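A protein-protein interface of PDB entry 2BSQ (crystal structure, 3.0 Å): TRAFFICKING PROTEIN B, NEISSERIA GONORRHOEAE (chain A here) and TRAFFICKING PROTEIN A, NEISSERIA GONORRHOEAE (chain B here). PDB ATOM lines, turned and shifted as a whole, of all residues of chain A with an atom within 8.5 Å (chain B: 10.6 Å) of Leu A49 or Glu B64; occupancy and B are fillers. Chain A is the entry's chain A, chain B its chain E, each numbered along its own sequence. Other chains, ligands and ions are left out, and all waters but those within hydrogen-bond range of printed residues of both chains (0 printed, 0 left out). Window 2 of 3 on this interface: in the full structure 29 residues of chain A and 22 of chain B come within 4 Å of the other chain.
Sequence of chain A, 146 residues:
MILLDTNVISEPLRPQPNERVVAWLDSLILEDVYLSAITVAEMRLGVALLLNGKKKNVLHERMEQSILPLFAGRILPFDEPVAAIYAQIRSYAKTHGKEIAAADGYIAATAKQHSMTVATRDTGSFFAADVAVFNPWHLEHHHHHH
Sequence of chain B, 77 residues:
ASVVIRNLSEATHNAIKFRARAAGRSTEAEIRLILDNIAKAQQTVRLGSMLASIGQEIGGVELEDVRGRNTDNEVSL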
ATOM      1  N   THR A   6       5.201  10.252  -0.857  1.00  0.00           N
ATOM      2  CA  THR A   6       5.522  11.340  -1.773  1.00  0.00           C
ATOM      3  C   THR A   6       5.329  11.057  -3.257  1.00  0.00           C
ATOM      4  O   THR A   6       4.545  11.733  -3.925  1.00  0.00           O
ATOM      5  CB  THR A   6       6.962  11.787  -1.576  1.00  0.00           C
ATOM      6  OG1 THR A   6       7.201  11.978  -0.181  1.00  0.00           O
ATOM      7  CG2 THR A   6       7.220  13.089  -2.303  1.00  0.00           C
ATOM      8  N   ASN A   7       6.037  10.063  -3.775  1.00  0.00           N
ATOM      9  CA  ASN A   7       5.954   9.743  -5.194  1.00  0.00           C
ATOM     10  C   ASN A   7       4.564   9.463  -5.777  1.00  0.00           C
ATOM     11  O   ASN A   7       4.371   9.582  -6.985  1.00  0.00           O
ATOM     12  CB  ASN A   7       6.915   8.597  -5.528  1.00  0.00           C
ATOM     13  CG  ASN A   7       6.512   7.295  -4.894  1.00  0.00           C
ATOM     14  OD1 ASN A   7       5.697   6.555  -5.442  1.00  0.00           O
ATOM     15  ND2 ASN A   7       7.071   7.008  -3.720  1.00  0.00           N
ATOM     16  N   SER A  10       2.643  12.812  -6.118  1.00  0.00           N
ATOM     17  CA  SER A  10       3.318  13.582  -7.161  1.00  0.00           C
ATOM     18  C   SER A  10       2.907  13.168  -8.561  1.00  0.00           C
ATOM     19  O   SER A  10       2.805  14.006  -9.460  1.00  0.00           O
ATOM     20  CB  SER A  10       4.832  13.405  -7.076  1.00  0.00           C
ATOM     21  OG  SER A  10       5.367  13.916  -5.879  1.00  0.00           O
ATOM     22  N   GLU A  42       8.703  16.910   2.309  1.00  0.00           N
ATOM     23  CA  GLU A  42       9.245  16.633   0.983  1.00  0.00           C
ATOM     24  C   GLU A  42       8.531  17.411  -0.124  1.00  0.00           C
ATOM     25  O   GLU A  42       9.169  18.010  -0.981  1.00  0.00           O
ATOM     26  CB  GLU A  42       9.171  15.135   0.692  1.00  0.00           C
ATOM     27  CG  GLU A  42      10.480  14.400   0.910  1.00  0.00           C
ATOM     28  CD  GLU A  42      10.329  12.883   0.847  1.00  0.00           C
ATOM     29  OE1 GLU A  42       9.734  12.354  -0.126  1.00  0.00           O
ATOM     30  OE2 GLU A  42      10.819  12.212   1.780  1.00  0.00           O
ATOM     31  N   MET A  43       7.204  17.397  -0.107  1.00  0.00           N
ATOM     32  CA  MET A  43       6.426  18.113  -1.106  1.00  0.00           C
ATOM     33  C   MET A  43       6.749  19.592  -1.018  1.00  0.00           C
ATOM     34  O   MET A  43       7.117  20.224  -2.009  1.00  0.00           O
ATOM     35  CB  MET A  43       4.937  17.937  -0.852  1.00  0.00           C
ATOM     36  CG  MET A  43       4.326  16.664  -1.380  1.00  0.00           C
ATOM     37  SD  MET A  43       2.644  16.473  -0.689  1.00  0.00           S
ATOM     38  CE  MET A  43       1.649  17.499  -1.814  1.00  0.00           C
ATOM     39  N   ARG A  44       6.598  20.141   0.181  1.00  0.00           N
ATOM     40  CA  ARG A  44       6.851  21.553   0.413  1.00  0.00           C
ATOM     41  C   ARG A  44       8.247  22.004  -0.031  1.00  0.00           C
ATOM     42  O   ARG A  44       8.409  23.122  -0.531  1.00  0.00           O
ATOM     43  CB  ARG A  44       6.619  21.873   1.888  1.00  0.00           C
ATOM     44  CG  ARG A  44       5.163  21.826   2.316  1.00  0.00           C
ATOM     45  CD  ARG A  44       4.676  23.215   2.574  1.00  0.00           C
ATOM     46  NE  ARG A  44       3.432  23.231   3.330  1.00  0.00           N
ATOM     47  CZ  ARG A  44       3.280  22.717   4.546  1.00  0.00           C
ATOM     48  NH1 ARG A  44       4.298  22.134   5.162  1.00  0.00           N
ATOM     49  NH2 ARG A  44       2.109  22.798   5.154  1.00  0.00           N
ATOM     50  N   LEU A  45       9.247  21.142   0.140  1.00  0.00           N
ATOM     51  CA  LEU A  45      10.616  21.465  -0.272  1.00  0.00           C
ATOM     52  C   LEU A  45      10.768  21.296  -1.779  1.00  0.00           C
ATOM     53  O   LEU A  45      11.477  22.056  -2.436  1.00  0.00           O
ATOM     54  CB  LEU A  45      11.635  20.558   0.432  1.00  0.00           C
ATOM     55  CG  LEU A  45      13.080  20.607  -0.082  1.00  0.00           C
ATOM     56  CD1 LEU A  45      13.573  22.022  -0.035  1.00  0.00           C
ATOM     57  CD2 LEU A  45      13.977  19.721   0.752  1.00  0.00           C
ATOM     58  N   GLY A  46      10.107  20.287  -2.325  1.00  0.00           N
ATOM     59  CA  GLY A  46      10.201  20.055  -3.753  1.00  0.00           C
ATOM     60  C   GLY A  46       9.694  21.240  -4.545  1.00  0.00           C
ATOM     61  O   GLY A  46      10.116  21.478  -5.679  1.00  0.00           O
ATOM     62  N   VAL A  47       8.763  21.976  -3.948  1.00  0.00           N
ATOM     63  CA  VAL A  47       8.200  23.143  -4.596  1.00  0.00           C
ATOM     64  C   VAL A  47       9.203  24.277  -4.433  1.00  0.00           C
ATOM     65  O   VAL A  47       9.642  24.877  -5.414  1.00  0.00           O
ATOM     66  CB  VAL A  47       6.848  23.527  -3.956  1.00  0.00           C
ATOM     67  CG1 VAL A  47       6.377  24.882  -4.468  1.00  0.00           C
ATOM     68  CG2 VAL A  47       5.820  22.468  -4.281  1.00  0.00           C
ATOM     69  N   ALA A  48       9.577  24.543  -3.187  1.00  0.00           N
ATOM     70  CA  ALA A  48      10.532  25.596  -2.873  1.00  0.00           C
ATOM     71  C   ALA A  48      11.796  25.598  -3.743  1.00  0.00           C
ATOM     72  O   ALA A  48      12.364  26.660  -4.016  1.00  0.00           O
ATOM     73  CB  ALA A  48      10.920  25.486  -1.419  1.00  0.00           C
ATOM     74  N   LEU A  49      12.233  24.419  -4.181  1.00  0.00           N
ATOM     75  CA  LEU A  49      13.446  24.309  -4.984  1.00  0.00           C
ATOM     76  C   LEU A  49      13.340  24.671  -6.462  1.00  0.00           C
ATOM     77  O   LEU A  49      14.350  24.678  -7.159  1.00  0.00           O
ATOM     78  CB  LEU A  49      14.032  22.901  -4.870  1.00  0.00           C
ATOM     79  CG  LEU A  49      14.658  22.471  -3.544  1.00  0.00           C
ATOM     80  CD1 LEU A  49      15.105  21.033  -3.647  1.00  0.00           C
ATOM     81  CD2 LEU A  49      15.839  23.347  -3.208  1.00  0.00           C
ATOM     82  N   LEU A  50      12.141  24.966  -6.947  1.00  0.00           N
ATOM     83  CA  LEU A  50      11.962  25.324  -8.356  1.00  0.00           C
ATOM     84  C   LEU A  50      12.457  26.742  -8.633  1.00  0.00           C
ATOM     85  O   LEU A  50      12.383  27.600  -7.744  1.00  0.00           O
ATOM     86  CB  LEU A  50      10.480  25.248  -8.737  1.00  0.00           C
ATOM     87  CG  LEU A  50       9.819  23.883  -8.934  1.00  0.00           C
ATOM     88  CD1 LEU A  50       8.337  24.077  -9.167  1.00  0.00           C
ATOM     89  CD2 LEU A  50      10.463  23.157 -10.109  1.00  0.00           C
ATOM     90  N   LEU A  51      12.953  26.998  -9.850  1.00  0.00           N
ATOM     91  CA  LEU A  51      13.416  28.341 -10.212  1.00  0.00           C
ATOM     92  C   LEU A  51      12.240  29.313 -10.114  1.00  0.00           C
ATOM     93  O   LEU A  51      11.118  29.008 -10.530  1.00  0.00           O
ATOM     94  CB  LEU A  51      13.965  28.387 -11.643  1.00  0.00           C
ATOM     95  CG  LEU A  51      15.185  27.548 -12.035  1.00  0.00           C
ATOM     96  CD1 LEU A  51      15.723  28.017 -13.376  1.00  0.00           C
ATOM     97  CD2 LEU A  51      16.258  27.676 -10.977  1.00  0.00           C
ATOM     98  N   ASN A  52      12.500  30.491  -9.569  1.00  0.00           N
ATOM     99  CA  ASN A  52      11.458  31.489  -9.408  1.00  0.00           C
ATOM    100  C   ASN A  52      10.801  31.890 -10.717  1.00  0.00           C
ATOM    101  O   ASN A  52      11.455  32.355 -11.646  1.00  0.00           O
ATOM    102  CB  ASN A  52      12.030  32.706  -8.690  1.00  0.00           C
ATOM    103  CG  ASN A  52      12.247  32.446  -7.211  1.00  0.00           C
ATOM    104  OD1 ASN A  52      11.324  32.589  -6.407  1.00  0.00           O
ATOM    105  ND2 ASN A  52      13.461  32.035  -6.845  1.00  0.00           N
ATOM    106  N   LYS A  56       6.042  28.112 -10.337  1.00  0.00           N
ATOM    107  CA  LYS A  56       6.285  27.866  -8.925  1.00  0.00           C
ATOM    108  C   LYS A  56       5.335  28.607  -7.996  1.00  0.00           C
ATOM    109  O   LYS A  56       5.025  28.115  -6.918  1.00  0.00           O
ATOM    110  CB  LYS A  56       7.729  28.212  -8.576  1.00  0.00           C
ATOM    111  CG  LYS A  56       8.004  28.247  -7.101  1.00  0.00           C
ATOM    112  CD  LYS A  56       9.465  28.490  -6.844  1.00  0.00           C
ATOM    113  CE  LYS A  56       9.698  28.870  -5.401  1.00  0.00           C
ATOM    114  NZ  LYS A  56      11.148  29.004  -5.110  1.00  0.00           N
ATOM    115  N   VAL B  61       4.610  19.285 -13.542  1.00  0.00           N
ATOM    116  CA  VAL B  61       5.881  19.525 -12.887  1.00  0.00           C
ATOM    117  C   VAL B  61       6.615  18.225 -12.709  1.00  0.00           C
ATOM    118  O   VAL B  61       6.071  17.146 -12.934  1.00  0.00           O
ATOM    119  CB  VAL B  61       5.719  20.126 -11.491  1.00  0.00           C
ATOM    120  CG1 VAL B  61       5.386  21.581 -11.598  1.00  0.00           C
ATOM    121  CG2 VAL B  61       4.642  19.382 -10.730  1.00  0.00           C
ATOM    122  N   GLU B  62       7.862  18.348 -12.292  1.00  0.00           N
ATOM    123  CA  GLU B  62       8.722  17.208 -12.042  1.00  0.00           C
ATOM    124  C   GLU B  62       9.541  17.618 -10.828  1.00  0.00           C
ATOM    125  O   GLU B  62      10.610  18.203 -10.959  1.00  0.00           O
ATOM    126  CB  GLU B  62       9.632  16.957 -13.250  1.00  0.00           C
ATOM    127  CG  GLU B  62       8.951  16.307 -14.458  1.00  0.00           C
ATOM    128  CD  GLU B  62       8.743  14.801 -14.290  1.00  0.00           C
ATOM    129  OE1 GLU B  62       9.138  14.259 -13.233  1.00  0.00           O
ATOM    130  OE2 GLU B  62       8.189  14.160 -15.215  1.00  0.00           O
ATOM    131  N   LEU B  63       9.022  17.339  -9.644  1.00  0.00           N
ATOM    132  CA  LEU B  63       9.724  17.707  -8.434  1.00  0.00           C
ATOM    133  C   LEU B  63      11.022  16.905  -8.315  1.00  0.00           C
ATOM    134  O   LEU B  63      11.120  15.787  -8.818  1.00  0.00           O
ATOM    135  CB  LEU B  63       8.818  17.459  -7.226  1.00  0.00           C
ATOM    136  CG  LEU B  63       7.414  18.048  -7.385  1.00  0.00           C
ATOM    137  CD1 LEU B  63       6.572  17.792  -6.135  1.00  0.00           C
ATOM    138  CD2 LEU B  63       7.530  19.533  -7.667  1.00  0.00           C
ATOM    139  N   GLU B  64      12.030  17.486  -7.672  1.00  0.00           N
ATOM    140  CA  GLU B  64      13.294  16.787  -7.498  1.00  0.00           C
ATOM    141  C   GLU B  64      13.016  15.611  -6.580  1.00  0.00           C
ATOM    142  O   GLU B  64      12.008  15.596  -5.877  1.00  0.00           O
ATOM    143  CB  GLU B  64      14.343  17.714  -6.874  1.00  0.00           C
ATOM    144  CG  GLU B  64      15.689  17.045  -6.599  1.00  0.00           C
ATOM    145  CD  GLU B  64      16.736  18.014  -6.078  1.00  0.00           C
ATOM    146  OE1 GLU B  64      17.695  17.557  -5.415  1.00  0.00           O
ATOM    147  OE2 GLU B  64      16.606  19.230  -6.338  1.00  0.00           O
ATOM    148  N   ASP B  65      13.903  14.623  -6.584  1.00  0.00           N
ATOM    149  CA  ASP B  65      13.699  13.452  -5.749  1.00  0.00           C
ATOM    150  C   ASP B  65      13.805  13.778  -4.266  1.00  0.00           C
ATOM    151  O   ASP B  65      12.805  13.727  -3.537  1.00  0.00           O
ATOM    152  CB  ASP B  65      14.696  12.342  -6.109  1.00  0.00           C
ATOM    153  CG  ASP B  65      14.284  10.972  -5.545  1.00  0.00           C
ATOM    154  OD1 ASP B  65      14.307  10.789  -4.303  1.00  0.00           O
ATOM    155  OD2 ASP B  65      13.929  10.080  -6.349  1.00  0.00           O
ATOM    156  N   VAL B  66      15.013  14.107  -3.823  1.00  0.00           N
ATOM    157  CA  VAL B  66      15.248  14.437  -2.420  1.00  0.00           C
ATOM    158  C   VAL B  66      14.869  13.284  -1.501  1.00  0.00           C
ATOM    159  O   VAL B  66      13.763  13.264  -0.958  1.00  0.00           O
ATOM    160  CB  VAL B  66      14.415  15.651  -1.966  1.00  0.00           C
ATOM    161  CG1 VAL B  66      14.847  16.069  -0.554  1.00  0.00           C
ATOM    162  CG2 VAL B  66      14.557  16.786  -2.966  1.00  0.00           C
ATOM    163  N   ARG B  67      15.782  12.334  -1.322  1.00  0.00           N
ATOM    164  CA  ARG B  67      15.530  11.186  -0.459  1.00  0.00           C
ATOM    165  C   ARG B  67      16.691  10.222  -0.604  1.00  0.00           C
ATOM    166  O   ARG B  67      16.864   9.599  -1.655  1.00  0.00           O
ATOM    167  CB  ARG B  67      14.220  10.498  -0.862  1.00  0.00           C
ATOM    168  CG  ARG B  67      13.636   9.521   0.161  1.00  0.00           C
ATOM    169  CD  ARG B  67      12.178   9.852   0.417  1.00  0.00           C
ATOM    170  NE  ARG B  67      11.429   8.745   1.004  1.00  0.00           N
ATOM    171  CZ  ARG B  67      10.131   8.797   1.294  1.00  0.00           C
ATOM    172  NH1 ARG B  67       9.433   9.902   1.060  1.00  0.00           N
ATOM    173  NH2 ARG B  67       9.525   7.736   1.807  1.00  0.00           N
ATOM    174  N   GLY B  68      17.482  10.111   0.460  1.00  0.00           N
ATOM    175  CA  GLY B  68      18.636   9.226   0.455  1.00  0.00           C
ATOM    176  C   GLY B  68      18.289   7.783   0.141  1.00  0.00           C
ATOM    177  O   GLY B  68      18.847   7.230  -0.835  1.00  0.00           O
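Among the printed residues, merely in contact across the chains: Glu A42 with Val B66 (3.9 Å), Leu A45 with Val B66 (3.97 Å), Gly A46 with Leu B63 (3.8 Å) and Leu A49 with Glu B64 (3.6 Å).
Of the 8 printed residues of chain B, 4 touch a printed residue of chain A. Hydrophobic or aromatic side chains of chain B that line the printed part of chain A: Leu B63 and Val B66. Printed residues of chain A that touch a printed residue of chain B: Thr A6, Glu A42, Leu A45, Gly A46 and Leu A49. Hydrophobic or aromatic side chains of chain A that line the printed part of chain B: Leu A45 and Leu A49. Among the printed residues, Asp or Glu carboxylates within 4 Å of a Lys or Arg side-chain nitrogen of the other chain: Glu A42 with Arg B67 (2.7 Å).
The guanidinium group of Arg B67 lies within hydrogen-bond range of the side-chain hydroxyl of Thr A6 (3.3 Å). OE1 of Glu A42 is in salt-bridge range of NH1 of Arg B67 (2.7 Å).
Leu A49 touches just one residue of chain B: Glu B64 (3.6 Å). Of chain A, only Leu A49 comes within 4 Å of Glu B64. Leu A45 touches one residue of chain B. Gly A46 touches just one residue of chain B: Leu B63. No residue of chain B comes within 4 Å of Ala A48. No residue of chain B comes within 4 Å of Leu A50. Of the printed residues of chain A, Val B66 touches Glu A42 and Leu A45. Printed residues of chain A within 4 Å of Arg B67: Thr A6 and Glu A42. Printed residues of chain B within 4 Å of Thr A6: Arg B67. Printed residues of chain A within 4 Å of Leu B63: Gly A46. Printed residues of chain B within 4 Å of Glu A42: Val B66 (3.9 Å) and Arg B67 (2.7 Å). Ser A10 touches none of the printed residues of chain B. Asp B65 touches none of the printed residues of chain A. The nearest residue of chain A that does not touch Glu B64 is Gly A46 (4.9 Å). The nearest printed residue of chain B that does not touch Thr A6 is Asp B65 (5.8 Å).
O of Thr A6 is in hydrogen-bond range of OG of Ser A10 (3.0 Å). The side-chain hydroxyl (OG1) of Thr A6 is in hydrogen-bond range of the side-chain carboxylate (OE1) of Glu A42, at 2.6 Å.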
